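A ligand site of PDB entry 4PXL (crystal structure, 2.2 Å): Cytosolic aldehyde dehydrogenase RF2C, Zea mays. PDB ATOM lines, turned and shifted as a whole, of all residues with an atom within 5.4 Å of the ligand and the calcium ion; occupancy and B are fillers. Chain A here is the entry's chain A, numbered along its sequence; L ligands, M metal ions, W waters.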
ATOM      1  N   ILE A 181      30.862  14.295  13.622  1.00  0.00           N
ATOM      2  CA  ILE A 181      30.883  12.870  13.953  1.00  0.00           C
ATOM      3  C   ILE A 181      29.433  12.502  14.225  1.00  0.00           C
ATOM      4  O   ILE A 181      28.798  13.045  15.121  1.00  0.00           O
ATOM      5  CB  ILE A 181      31.864  12.541  15.106  1.00  0.00           C
ATOM      6  CG1 ILE A 181      33.308  12.993  14.740  1.00  0.00           C
ATOM      7  CG2 ILE A 181      31.831  11.056  15.434  1.00  0.00           C
ATOM      8  CD1 ILE A 181      34.273  13.128  15.896  1.00  0.00           C
ATOM      9  N   VAL A 182      28.867  11.642  13.384  1.00  0.00           N
ATOM     10  CA  VAL A 182      27.431  11.339  13.488  1.00  0.00           C
ATOM     11  C   VAL A 182      27.092   9.893  13.850  1.00  0.00           C
ATOM     12  O   VAL A 182      27.890   9.003  13.491  1.00  0.00           O
ATOM     13  CB  VAL A 182      26.669  11.839  12.228  1.00  0.00           C
ATOM     14  CG1 VAL A 182      26.513  13.355  12.259  1.00  0.00           C
ATOM     15  CG2 VAL A 182      27.359  11.426  10.957  1.00  0.00           C
ATOM     16  N   PRO A 183      25.938   9.645  14.544  1.00  0.00           N
ATOM     17  CA  PRO A 183      25.568   8.261  14.874  1.00  0.00           C
ATOM     18  C   PRO A 183      24.740   7.589  13.764  1.00  0.00           C
ATOM     19  O   PRO A 183      24.452   8.188  12.727  1.00  0.00           O
ATOM     20  CB  PRO A 183      24.755   8.432  16.150  1.00  0.00           C
ATOM     21  CG  PRO A 183      24.023   9.704  15.929  1.00  0.00           C
ATOM     22  CD  PRO A 183      24.943  10.587  15.099  1.00  0.00           C
ATOM     23  N   TRP A 184      24.299   6.365  14.012  1.00  0.00           N
ATOM     24  CA  TRP A 184      23.580   5.509  13.062  1.00  0.00           C
ATOM     25  C   TRP A 184      22.045   5.536  13.119  1.00  0.00           C
ATOM     26  O   TRP A 184      21.408   5.002  12.205  1.00  0.00           O
ATOM     27  CB  TRP A 184      24.046   4.058  13.239  1.00  0.00           C
ATOM     28  CG  TRP A 184      24.127   3.633  14.684  1.00  0.00           C
ATOM     29  CD1 TRP A 184      25.243   3.612  15.465  1.00  0.00           C
ATOM     30  CD2 TRP A 184      23.043   3.235  15.537  1.00  0.00           C
ATOM     31  NE1 TRP A 184      24.923   3.213  16.743  1.00  0.00           N
ATOM     32  CE2 TRP A 184      23.587   2.962  16.814  1.00  0.00           C
ATOM     33  CE3 TRP A 184      21.662   3.064  15.347  1.00  0.00           C
ATOM     34  CZ2 TRP A 184      22.801   2.537  17.896  1.00  0.00           C
ATOM     35  CZ3 TRP A 184      20.876   2.670  16.422  1.00  0.00           C
ATOM     36  CH2 TRP A 184      21.447   2.394  17.674  1.00  0.00           C
ATOM     37  N   ASN A 185      21.452   6.079  14.195  1.00  0.00           N
ATOM     38  CA  ASN A 185      20.005   5.979  14.370  1.00  0.00           C
ATOM     39  C   ASN A 185      19.115   6.712  13.377  1.00  0.00           C
ATOM     40  O   ASN A 185      18.098   6.163  12.945  1.00  0.00           O
ATOM     41  CB  ASN A 185      19.588   6.175  15.841  1.00  0.00           C
ATOM     42  CG  ASN A 185      19.823   7.560  16.358  1.00  0.00           C
ATOM     43  OD1 ASN A 185      20.908   8.125  16.234  1.00  0.00           O
ATOM     44  ND2 ASN A 185      18.792   8.130  16.946  1.00  0.00           N
ATOM     45  N   MET A 190      20.599  13.312  11.060  1.00  0.00           N
ATOM     46  CA  MET A 190      21.820  13.711  11.769  1.00  0.00           C
ATOM     47  C   MET A 190      22.799  14.388  10.840  1.00  0.00           C
ATOM     48  O   MET A 190      23.391  15.389  11.224  1.00  0.00           O
ATOM     49  CB  MET A 190      22.485  12.505  12.427  1.00  0.00           C
ATOM     50  CG  MET A 190      21.667  11.862  13.511  1.00  0.00           C
ATOM     51  SD  MET A 190      21.490  12.975  14.885  1.00  0.00           S
ATOM     52  CE  MET A 190      19.734  13.190  14.853  1.00  0.00           C
ATOM     53  N   LYS A 208      32.174  12.400   9.405  1.00  0.00           N
ATOM     54  CA  LYS A 208      32.546  11.037   9.696  1.00  0.00           C
ATOM     55  C   LYS A 208      31.262  10.306  10.095  1.00  0.00           C
ATOM     56  O   LYS A 208      30.804  10.416  11.238  1.00  0.00           O
ATOM     57  CB  LYS A 208      33.652  10.944  10.776  1.00  0.00           C
ATOM     58  CG  LYS A 208      34.577   9.725  10.624  1.00  0.00           C
ATOM     59  CD  LYS A 208      33.930   8.333  10.824  1.00  0.00           C
ATOM     60  CE  LYS A 208      33.347   8.069  12.202  1.00  0.00           C
ATOM     61  NZ  LYS A 208      32.585   6.792  12.224  1.00  0.00           N
ATOM     62  N   PRO A 209      30.640   9.593   9.131  1.00  0.00           N
ATOM     63  CA  PRO A 209      29.389   8.878   9.458  1.00  0.00           C
ATOM     64  C   PRO A 209      29.690   7.607  10.230  1.00  0.00           C
ATOM     65  O   PRO A 209      30.829   7.125  10.192  1.00  0.00           O
ATOM     66  CB  PRO A 209      28.764   8.602   8.090  1.00  0.00           C
ATOM     67  CG  PRO A 209      29.932   8.485   7.161  1.00  0.00           C
ATOM     68  CD  PRO A 209      31.032   9.374   7.722  1.00  0.00           C
ATOM     69  N   ALA A 210      28.695   7.075  10.949  1.00  0.00           N
ATOM     70  CA  ALA A 210      28.800   5.850  11.746  1.00  0.00           C
ATOM     71  C   ALA A 210      29.146   4.677  10.826  1.00  0.00           C
ATOM     72  O   ALA A 210      28.652   4.635   9.700  1.00  0.00           O
ATOM     73  CB  ALA A 210      27.462   5.570  12.429  1.00  0.00           C
ATOM     74  N   GLU A 211      29.996   3.747  11.298  1.00  0.00           N
ATOM     75  CA  GLU A 211      30.390   2.547  10.549  1.00  0.00           C
ATOM     76  C   GLU A 211      29.172   1.684  10.176  1.00  0.00           C
ATOM     77  O   GLU A 211      29.128   1.107   9.096  1.00  0.00           O
ATOM     78  CB  GLU A 211      31.497   1.733  11.277  1.00  0.00           C
ATOM     79  CG  GLU A 211      31.199   1.345  12.732  1.00  0.00           C
ATOM     80  CD  GLU A 211      31.498   2.371  13.807  1.00  0.00           C
ATOM     81  OE1 GLU A 211      31.846   1.954  14.940  1.00  0.00           O
ATOM     82  OE2 GLU A 211      31.353   3.595  13.551  1.00  0.00           O
ATOM     83  N   GLN A 212      28.141   1.692  11.032  1.00  0.00           N
ATOM     84  CA  GLN A 212      26.898   0.965  10.817  1.00  0.00           C
ATOM     85  C   GLN A 212      26.065   1.570   9.681  1.00  0.00           C
ATOM     86  O   GLN A 212      25.280   0.855   9.056  1.00  0.00           O
ATOM     87  CB  GLN A 212      26.025   0.943  12.098  1.00  0.00           C
ATOM     88  CG  GLN A 212      26.682   0.204  13.267  1.00  0.00           C
ATOM     89  CD  GLN A 212      27.434   1.133  14.204  1.00  0.00           C
ATOM     90  OE1 GLN A 212      27.857   2.249  13.848  1.00  0.00           O
ATOM     91  NE2 GLN A 212      27.668   0.660  15.421  1.00  0.00           N
ATOM     92  N   GLY A 239      34.228   5.207   8.117  1.00  0.00           N
ATOM     93  CA  GLY A 239      35.281   4.508   8.845  1.00  0.00           C
ATOM     94  C   GLY A 239      34.922   4.315  10.301  1.00  0.00           C
ATOM     95  O   GLY A 239      33.857   4.751  10.739  1.00  0.00           O
ATOM     96  N   PHE A 240      35.810   3.666  11.059  1.00  0.00           N
ATOM     97  CA  PHE A 240      35.575   3.389  12.487  1.00  0.00           C
ATOM     98  C   PHE A 240      35.775   4.598  13.400  1.00  0.00           C
ATOM     99  O   PHE A 240      36.367   5.595  12.995  1.00  0.00           O
ATOM    100  CB  PHE A 240      36.346   2.147  12.941  1.00  0.00           C
ATOM    101  CG  PHE A 240      35.985   0.934  12.123  1.00  0.00           C
ATOM    102  CD1 PHE A 240      34.751   0.302  12.294  1.00  0.00           C
ATOM    103  CD2 PHE A 240      36.867   0.420  11.174  1.00  0.00           C
ATOM    104  CE1 PHE A 240      34.411  -0.815  11.523  1.00  0.00           C
ATOM    105  CE2 PHE A 240      36.518  -0.706  10.409  1.00  0.00           C
ATOM    106  CZ  PHE A 240      35.296  -1.310  10.586  1.00  0.00           C
ATOM    107  N   GLY A 241      35.222   4.511  14.602  1.00  0.00           N
ATOM    108  CA  GLY A 241      35.271   5.583  15.581  1.00  0.00           C
ATOM    109  C   GLY A 241      36.635   5.884  16.176  1.00  0.00           C
ATOM    110  O   GLY A 241      37.086   7.022  16.058  1.00  0.00           O
ATOM    111  N   PRO A 242      37.311   4.906  16.829  1.00  0.00           N
ATOM    112  CA  PRO A 242      38.625   5.187  17.430  1.00  0.00           C
ATOM    113  C   PRO A 242      39.742   5.527  16.455  1.00  0.00           C
ATOM    114  O   PRO A 242      40.813   5.966  16.895  1.00  0.00           O
ATOM    115  CB  PRO A 242      38.942   3.891  18.179  1.00  0.00           C
ATOM    116  CG  PRO A 242      37.590   3.223  18.389  1.00  0.00           C
ATOM    117  CD  PRO A 242      36.895   3.517  17.110  1.00  0.00           C
ATOM    118  N   GLY A 245      37.065   8.710  13.480  1.00  0.00           N
ATOM    119  CA  GLY A 245      36.326   9.606  14.350  1.00  0.00           C
ATOM    120  C   GLY A 245      37.240  10.332  15.311  1.00  0.00           C
ATOM    121  O   GLY A 245      37.106  11.539  15.506  1.00  0.00           O
ATOM    122  N   ALA A 246      38.195   9.597  15.899  1.00  0.00           N
ATOM    123  CA  ALA A 246      39.161  10.176  16.845  1.00  0.00           C
ATOM    124  C   ALA A 246      40.099  11.137  16.130  1.00  0.00           C
ATOM    125  O   ALA A 246      40.453  12.171  16.715  1.00  0.00           O
ATOM    126  CB  ALA A 246      39.954   9.064  17.523  1.00  0.00           C
ATOM    127  N   ALA A 249      38.245  14.570  15.836  1.00  0.00           N
ATOM    128  CA  ALA A 249      38.188  15.185  17.165  1.00  0.00           C
ATOM    129  C   ALA A 249      39.549  15.763  17.600  1.00  0.00           C
ATOM    130  O   ALA A 249      39.582  16.842  18.170  1.00  0.00           O
ATOM    131  CB  ALA A 249      37.715  14.146  18.195  1.00  0.00           C
ATOM    132  N   PHE A 259      29.521  16.506  17.789  1.00  0.00           N
ATOM    133  CA  PHE A 259      29.389  15.078  18.016  1.00  0.00           C
ATOM    134  C   PHE A 259      27.982  14.751  18.560  1.00  0.00           C
ATOM    135  O   PHE A 259      27.410  15.493  19.379  1.00  0.00           O
ATOM    136  CB  PHE A 259      30.483  14.594  18.998  1.00  0.00           C
ATOM    137  CG  PHE A 259      30.279  13.203  19.552  1.00  0.00           C
ATOM    138  CD1 PHE A 259      30.767  12.084  18.882  1.00  0.00           C
ATOM    139  CD2 PHE A 259      29.524  12.997  20.712  1.00  0.00           C
ATOM    140  CE1 PHE A 259      30.477  10.793  19.332  1.00  0.00           C
ATOM    141  CE2 PHE A 259      29.267  11.719  21.185  1.00  0.00           C
ATOM    142  CZ  PHE A 259      29.753  10.621  20.491  1.00  0.00           C
ATOM    143  N   THR A 260      27.443  13.643  18.069  1.00  0.00           N
ATOM    144  CA  THR A 260      26.174  13.089  18.515  1.00  0.00           C
ATOM    145  C   THR A 260      26.419  11.596  18.725  1.00  0.00           C
ATOM    146  O   THR A 260      26.947  10.937  17.830  1.00  0.00           O
ATOM    147  CB  THR A 260      25.036  13.420  17.570  1.00  0.00           C
ATOM    148  OG1 THR A 260      24.976  14.840  17.433  1.00  0.00           O
ATOM    149  CG2 THR A 260      23.692  12.872  18.069  1.00  0.00           C
ATOM    150  N   GLY A 261      26.093  11.093  19.901  1.00  0.00           N
ATOM    151  CA  GLY A 261      26.292   9.693  20.192  1.00  0.00           C
ATOM    152  C   GLY A 261      26.291   9.364  21.663  1.00  0.00           C
ATOM    153  O   GLY A 261      25.554   9.971  22.431  1.00  0.00           O
ATOM    154  N   SER A 262      27.098   8.394  22.047  1.00  0.00           N
ATOM    155  CA  SER A 262      27.131   7.936  23.436  1.00  0.00           C
ATOM    156  C   SER A 262      27.853   8.902  24.356  1.00  0.00           C
ATOM    157  O   SER A 262      28.749   9.617  23.918  1.00  0.00           O
ATOM    158  CB  SER A 262      27.754   6.541  23.546  1.00  0.00           C
ATOM    159  OG  SER A 262      29.148   6.563  23.296  1.00  0.00           O
ATOM    160  N   VAL A 265      31.820   8.273  24.527  1.00  0.00           N
ATOM    161  CA  VAL A 265      32.589   8.818  23.414  1.00  0.00           C
ATOM    162  C   VAL A 265      32.588  10.351  23.471  1.00  0.00           C
ATOM    163  O   VAL A 265      33.589  10.977  23.116  1.00  0.00           O
ATOM    164  CB  VAL A 265      32.139   8.211  22.049  1.00  0.00           C
ATOM    165  CG1 VAL A 265      32.827   8.890  20.870  1.00  0.00           C
ATOM    166  CG2 VAL A 265      32.406   6.699  22.023  1.00  0.00           C
ATOM    167  N   LEU A 268      35.425  11.427  25.301  1.00  0.00           N
ATOM    168  CA  LEU A 268      36.621  11.243  24.477  1.00  0.00           C
ATOM    169  C   LEU A 268      36.801  12.370  23.486  1.00  0.00           C
ATOM    170  O   LEU A 268      37.904  12.881  23.368  1.00  0.00           O
ATOM    171  CB  LEU A 268      36.629   9.862  23.784  1.00  0.00           C
ATOM    172  CG  LEU A 268      36.648   8.641  24.708  1.00  0.00           C
ATOM    173  CD1 LEU A 268      36.556   7.343  23.900  1.00  0.00           C
ATOM    174  CD2 LEU A 268      37.871   8.623  25.635  1.00  0.00           C
ATOM    175  N   VAL A 269      35.697  12.832  22.867  1.00  0.00           N
ATOM    176  CA  VAL A 269      35.671  13.955  21.931  1.00  0.00           C
ATOM    177  C   VAL A 269      36.044  15.255  22.639  1.00  0.00           C
ATOM    178  O   VAL A 269      36.905  15.987  22.149  1.00  0.00           O
ATOM    179  CB  VAL A 269      34.346  14.039  21.144  1.00  0.00           C
ATOM    180  CG1 VAL A 269      34.244  15.348  20.332  1.00  0.00           C
ATOM    181  CG2 VAL A 269      34.188  12.815  20.244  1.00  0.00           C
ATOM    182  N   GLU A 284      25.607  16.041  21.688  1.00  0.00           N
ATOM    183  CA  GLU A 284      24.254  15.505  21.926  1.00  0.00           C
ATOM    184  C   GLU A 284      24.518  14.061  22.361  1.00  0.00           C
ATOM    185  O   GLU A 284      25.019  13.253  21.568  1.00  0.00           O
ATOM    186  CB  GLU A 284      23.325  15.611  20.707  1.00  0.00           C
ATOM    187  CG  GLU A 284      21.851  15.384  21.064  1.00  0.00           C
ATOM    188  CD  GLU A 284      21.395  13.936  21.024  1.00  0.00           C
ATOM    189  OE1 GLU A 284      20.917  13.488  19.956  1.00  0.00           O
ATOM    190  OE2 GLU A 284      21.535  13.227  22.054  1.00  0.00           O
ATOM    191  N   LEU A 285      24.297  13.784  23.647  1.00  0.00           N
ATOM    192  CA  LEU A 285      24.673  12.531  24.270  1.00  0.00           C
ATOM    193  C   LEU A 285      23.552  11.597  24.693  1.00  0.00           C
ATOM    194  O   LEU A 285      23.785  10.627  25.429  1.00  0.00           O
ATOM    195  CB  LEU A 285      25.637  12.819  25.430  1.00  0.00           C
ATOM    196  CG  LEU A 285      26.807  13.717  25.102  1.00  0.00           C
ATOM    197  CD1 LEU A 285      27.583  14.080  26.339  1.00  0.00           C
ATOM    198  CD2 LEU A 285      27.710  13.087  24.031  1.00  0.00           C
ATOM    199  N   GLY A 286      22.347  11.841  24.180  1.00  0.00           N
ATOM    200  CA  GLY A 286      21.239  10.950  24.518  1.00  0.00           C
ATOM    201  C   GLY A 286      20.603  11.257  25.865  1.00  0.00           C
ATOM    202  O   GLY A 286      20.973  12.214  26.538  1.00  0.00           O
ATOM    203  N   CSO A 318      17.535   9.215  20.879  1.00  0.00           N
ATOM    204  CA  CSO A 318      18.068   9.913  22.039  1.00  0.00           C
ATOM    205  CB  CSO A 318      18.992  11.032  21.480  1.00  0.00           C
ATOM    206  SG  CSO A 318      18.066  12.227  20.388  1.00  0.00           S
ATOM    207  C   CSO A 318      16.952  10.496  22.935  1.00  0.00           C
ATOM    208  O   CSO A 318      17.167  10.655  24.128  1.00  0.00           O
ATOM    209  OD  CSO A 318      18.284  11.651  18.862  1.00  0.00           O
ATOM    210  N   ASP A 364      25.472  -5.872  18.350  1.00  0.00           N
ATOM    211  CA  ASP A 364      25.843  -5.245  19.633  1.00  0.00           C
ATOM    212  C   ASP A 364      24.661  -4.570  20.346  1.00  0.00           C
ATOM    213  O   ASP A 364      24.475  -4.769  21.547  1.00  0.00           O
ATOM    214  CB  ASP A 364      27.019  -4.246  19.479  1.00  0.00           C
ATOM    215  CG  ASP A 364      27.445  -3.610  20.795  1.00  0.00           C
ATOM    216  OD1 ASP A 364      28.144  -4.289  21.587  1.00  0.00           O
ATOM    217  OD2 ASP A 364      27.044  -2.449  21.056  1.00  0.00           O
ATOM    218  N   GLN A 365      23.862  -3.777  19.596  1.00  0.00           N
ATOM    219  CA  GLN A 365      22.696  -3.064  20.076  1.00  0.00           C
ATOM    220  C   GLN A 365      21.609  -4.029  20.547  1.00  0.00           C
ATOM    221  O   GLN A 365      21.087  -3.886  21.646  1.00  0.00           O
ATOM    222  CB  GLN A 365      22.168  -2.112  18.974  1.00  0.00           C
ATOM    223  CG  GLN A 365      21.270  -0.984  19.488  1.00  0.00           C
ATOM    224  CD  GLN A 365      21.857  -0.225  20.653  1.00  0.00           C
ATOM    225  OE1 GLN A 365      23.082   0.076  20.731  1.00  0.00           O
ATOM    226  NE2 GLN A 365      21.004   0.063  21.611  1.00  0.00           N
ATOM    227  N   LYS A 368      22.798  -5.703  23.727  1.00  0.00           N
ATOM    228  CA  LYS A 368      22.762  -4.697  24.793  1.00  0.00           C
ATOM    229  C   LYS A 368      21.300  -4.532  25.329  1.00  0.00           C
ATOM    230  O   LYS A 368      21.099  -4.478  26.549  1.00  0.00           O
ATOM    231  CB  LYS A 368      23.291  -3.345  24.284  1.00  0.00           C
ATOM    232  CG  LYS A 368      23.542  -2.311  25.373  1.00  0.00           C
ATOM    233  CD  LYS A 368      23.628  -0.891  24.831  1.00  0.00           C
ATOM    234  CE  LYS A 368      24.043   0.102  25.885  1.00  0.00           C
ATOM    235  NZ  LYS A 368      25.016   1.104  25.362  1.00  0.00           N
ATOM    236  N   GLU A 415      20.377   4.573  29.794  1.00  0.00           N
ATOM    237  CA  GLU A 415      19.756   4.654  28.464  1.00  0.00           C
ATOM    238  C   GLU A 415      19.866   3.283  27.785  1.00  0.00           C
ATOM    239  O   GLU A 415      20.966   2.762  27.600  1.00  0.00           O
ATOM    240  CB  GLU A 415      20.412   5.744  27.599  1.00  0.00           C
ATOM    241  CG  GLU A 415      19.898   5.800  26.163  1.00  0.00           C
ATOM    242  CD  GLU A 415      20.507   6.912  25.316  1.00  0.00           C
ATOM    243  OE1 GLU A 415      19.744   7.637  24.647  1.00  0.00           O
ATOM    244  OE2 GLU A 415      21.757   7.056  25.342  1.00  0.00           O
ATOM    245  N   ILE A 416      18.711   2.690  27.480  1.00  0.00           N
ATOM    246  CA  ILE A 416      18.661   1.355  26.886  1.00  0.00           C
ATOM    247  C   ILE A 416      18.783   1.393  25.367  1.00  0.00           C
ATOM    248  O   ILE A 416      19.426   0.506  24.797  1.00  0.00           O
ATOM    249  CB  ILE A 416      17.407   0.562  27.398  1.00  0.00           C
ATOM    250  CG1 ILE A 416      17.449   0.460  28.964  1.00  0.00           C
ATOM    251  CG2 ILE A 416      17.286  -0.846  26.739  1.00  0.00           C
ATOM    252  CD1 ILE A 416      16.169  -0.104  29.673  1.00  0.00           C
ATOM    253  N   PHE A 417      18.178   2.403  24.709  1.00  0.00           N
ATOM    254  CA  PHE A 417      18.153   2.592  23.253  1.00  0.00           C
ATOM    255  C   PHE A 417      17.484   1.395  22.552  1.00  0.00           C
ATOM    256  O   PHE A 417      17.965   0.874  21.537  1.00  0.00           O
ATOM    257  CB  PHE A 417      19.572   2.896  22.732  1.00  0.00           C
ATOM    258  CG  PHE A 417      19.676   4.100  21.835  1.00  0.00           C
ATOM    259  CD1 PHE A 417      19.449   5.381  22.339  1.00  0.00           C
ATOM    260  CD2 PHE A 417      20.020   3.969  20.498  1.00  0.00           C
ATOM    261  CE1 PHE A 417      19.557   6.499  21.514  1.00  0.00           C
ATOM    262  CE2 PHE A 417      20.128   5.097  19.669  1.00  0.00           C
ATOM    263  CZ  PHE A 417      19.911   6.345  20.178  1.00  0.00           C
HETATM  264  P1  LIG L   1      29.125   5.852  19.637  1.00  0.00           P
HETATM  265  O1  LIG L   1      29.087   6.965  20.628  1.00  0.00           O
HETATM  266  O2  LIG L   1      30.271   4.924  19.866  1.00  0.00           O
HETATM  267  O3  LIG L   1      29.213   6.351  18.137  1.00  0.00           O
HETATM  268  C1  LIG L   1      28.753   7.593  17.579  1.00  0.00           C
HETATM  269  C2  LIG L   1      29.757   8.042  16.534  1.00  0.00           C
HETATM  270  O4  LIG L   1      31.032   8.295  17.168  1.00  0.00           O
HETATM  271  C3  LIG L   1      30.047   7.090  15.377  1.00  0.00           C
HETATM  272  O5  LIG L   1      30.217   7.790  14.144  1.00  0.00           O
HETATM  273  C4  LIG L   1      31.331   6.394  15.825  1.00  0.00           C
HETATM  274  O6  LIG L   1      32.109   5.817  14.788  1.00  0.00           O
HETATM  275  C5  LIG L   1      32.047   7.552  16.519  1.00  0.00           C
HETATM  276  N1  LIG L   1      33.048   7.173  17.524  1.00  0.00           N
HETATM  277  C6  LIG L   1      33.118   6.017  18.240  1.00  0.00           C
HETATM  278  N2  LIG L   1      34.187   5.924  18.999  1.00  0.00           N
HETATM  279  C7  LIG L   1      34.843   7.118  18.796  1.00  0.00           C
HETATM  280  C8  LIG L   1      36.024   7.667  19.343  1.00  0.00           C
HETATM  281  N3  LIG L   1      36.819   6.996  20.186  1.00  0.00           N
HETATM  282  N4  LIG L   1      36.370   8.914  18.957  1.00  0.00           N
HETATM  283  C9  LIG L   1      35.599   9.564  18.077  1.00  0.00           C
HETATM  284  N5  LIG L   1      34.489   9.143  17.468  1.00  0.00           N
HETATM  285  C10 LIG L   1      34.147   7.911  17.881  1.00  0.00           C
HETATM  286  O7  LIG L   1      27.806   4.941  19.726  1.00  0.00           O
HETATM  287  P2  LIG L   1      27.672   3.359  19.565  1.00  0.00           P
HETATM  288  O8  LIG L   1      29.013   2.723  19.517  1.00  0.00           O
HETATM  289  O9  LIG L   1      26.744   3.095  18.444  1.00  0.00           O
HETATM  290  O10 LIG L   1      26.973   2.985  20.954  1.00  0.00           O
HETATM  291  C11 LIG L   1      25.585   2.652  21.045  1.00  0.00           C
HETATM  292  C12 LIG L   1      24.982   3.342  22.235  1.00  0.00           C
HETATM  293  O11 LIG L   1      25.316   4.755  22.197  1.00  0.00           O
HETATM  294  C13 LIG L   1      23.452   3.291  22.277  1.00  0.00           C
HETATM  295  O12 LIG L   1      23.033   2.209  23.092  1.00  0.00           O
HETATM  296  C14 LIG L   1      23.085   4.666  22.828  1.00  0.00           C
HETATM  297  O13 LIG L   1      23.026   4.668  24.256  1.00  0.00           O
HETATM  298  C15 LIG L   1      24.246   5.616  22.390  1.00  0.00           C
HETATM  299  N6  LIG L   1      23.913   6.369  21.061  1.00  0.00           N
HETATM  300  C16 LIG L   1      23.366   7.657  21.223  1.00  0.00           C
HETATM  301  C17 LIG L   1      22.836   8.341  20.137  1.00  0.00           C
HETATM  302  C18 LIG L   1      22.314   9.756  20.279  1.00  0.00           C
HETATM  303  O14 LIG L   1      21.583  10.237  19.386  1.00  0.00           O
HETATM  304  N7  LIG L   1      22.558  10.398  21.409  1.00  0.00           N
HETATM  305  C19 LIG L   1      22.871   7.731  18.877  1.00  0.00           C
HETATM  306  C20 LIG L   1      23.471   6.482  18.720  1.00  0.00           C
HETATM  307  C21 LIG L   1      24.005   5.822  19.827  1.00  0.00           C
HETATM  308 CA    CA M   1      31.154   2.607  20.495  1.00  0.00          CA
HETATM  309  O   HOH W   1      28.866   3.938  15.798  1.00  0.00           O
HETATM  310  O   HOH W   2      39.471   7.707  21.008  1.00  0.00           O
HETATM  311  O   HOH W   3      30.881   3.097  17.423  1.00  0.00           O
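N7 of the ligand lies close to N of Gly 286 (3.1 Å). Ile 181 touches the ligand. CB of Pro 183 touches C19 of the ligand (3.4 Å). Asn 185 touches the ligand. Pro 209 touches the ligand. CA of Ala 210 touches O5 of the ligand, at 3.4 Å. NE2 of Gln 212 touches O9 of the ligand, at 3.99 Å. Pro 242 touches the ligand. C of Gly 245 touches C9 of the ligand, 3.3 Å away. Ala 246 touches the ligand. Phe 259 touches the ligand (CE1 to O4, 3.4 Å). Thr 260 touches the ligand (CG2 to O14, 3.6 Å). CG1 of Val 265 touches C7 of the ligand, at 3.4 Å. Leu 268 touches the ligand (CD1 to N3, 3.7 Å). C of Leu 285 touches N7 of the ligand (3.6 Å). CSO 318 touches the ligand. CZ of Phe 417 touches C19 of the ligand, at 3.5 Å. Hydrophobic or aromatic side chains that line the ligand: Ile 181, Pro 183, Trp 184, Ala 210, Ala 246, Phe 259, Val 265, Leu 268 and Phe 417. Within 4 Å of the ligand: Ile 181, Val 182, Pro 183, Trp 184, Asn 185, Lys 208, Pro 209, Ala 210, Glu 211, Gln 212, Gly 241, Pro 242, Gly 245, Ala 246, Phe 259, Thr 260, Gly 261, Ser 262, Val 265, Leu 268, Glu 284, Leu 285, Gly 286, CSO 318, Gln 365, Lys 368, Glu 415 and Phe 417.
No residue comes within 4 Å of the calcium ion. The nearest printed residue that does not touch the calcium ion is Val 265 (4.5 Å).
The side-chain amide oxygen (OE1) of Gln 365 sits at hydrogen-bond distance from an oxygen (O12) of the ligand (3.2 Å). The backbone NH of Gly 241 lies close to an oxygen (O6) of the ligand (3.4 Å). OG of Ser 262 lies within hydrogen-bond range of O1 of the ligand (2.7 Å). O of Gly 261 lies within hydrogen-bond range of N7 of the ligand (3.2 Å). The side-chain carboxylate (OE2) of Glu 284 sits at hydrogen-bond distance from a nitrogen (N7) of the ligand. An oxygen (O6) of the ligand lies within hydrogen-bond range of the side-chain amino group (NZ) of Lys 208. O5 of the ligand is in hydrogen-bond range of O of Val 182 (2.7 Å). An oxygen (O9) of the ligand lies within hydrogen-bond range of the indole nitrogen of Trp 184 (2.5 Å). An oxygen (O1) of the ligand lies within hydrogen-bond range of the backbone NH of Ser 262. The side-chain carboxylate of Glu 211 lies within hydrogen-bond range of an oxygen (O6) of the ligand. OE2 of Glu 415 is in hydrogen-bond range of O13 of the ligand (2.9 Å). The side-chain amino group (NZ) of Lys 368 sits at hydrogen-bond distance from an oxygen (O12) of the ligand (3.2 Å).
O of Phe 240 lies within hydrogen-bond range of N of Gly 245 (3.2 Å). The side-chain hydroxyl (OG) of Ser 262 lies within hydrogen-bond range of the backbone NH (N) of Val 265. The backbone NH of Ala 246 lies within hydrogen-bond range of the backbone carbonyl oxygen of Gly 241 (2.8 Å). The side-chain carboxylate (OE2) of Glu 284 lies within hydrogen-bond range of the backbone NH (N) of Gly 286 (2.7 Å). The backbone NH (N) of Thr 260 sits at hydrogen-bond distance from the backbone carbonyl oxygen (O) of Ile 181 (3.3 Å). O of Phe 259 is in hydrogen-bond range of N of Glu 284 (3.0 Å). OD of CSO 318 sits at hydrogen-bond distance from the side-chain carboxylate of Glu 284 (3.4 Å). The side-chain amino group (NZ) of Lys 208 lies within hydrogen-bond range of the backbone carbonyl oxygen (O) of Gly 239, at 2.8 Å.
The calcium ion is bound by an oxygen (O8) of the ligand (2.4 Å) and an oxygen (O2) of the ligand (2.6 Å). The calcium ion has two donor atoms within binding distance. Slightly farther from the calcium ion lies water W3 (3.1 Å).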
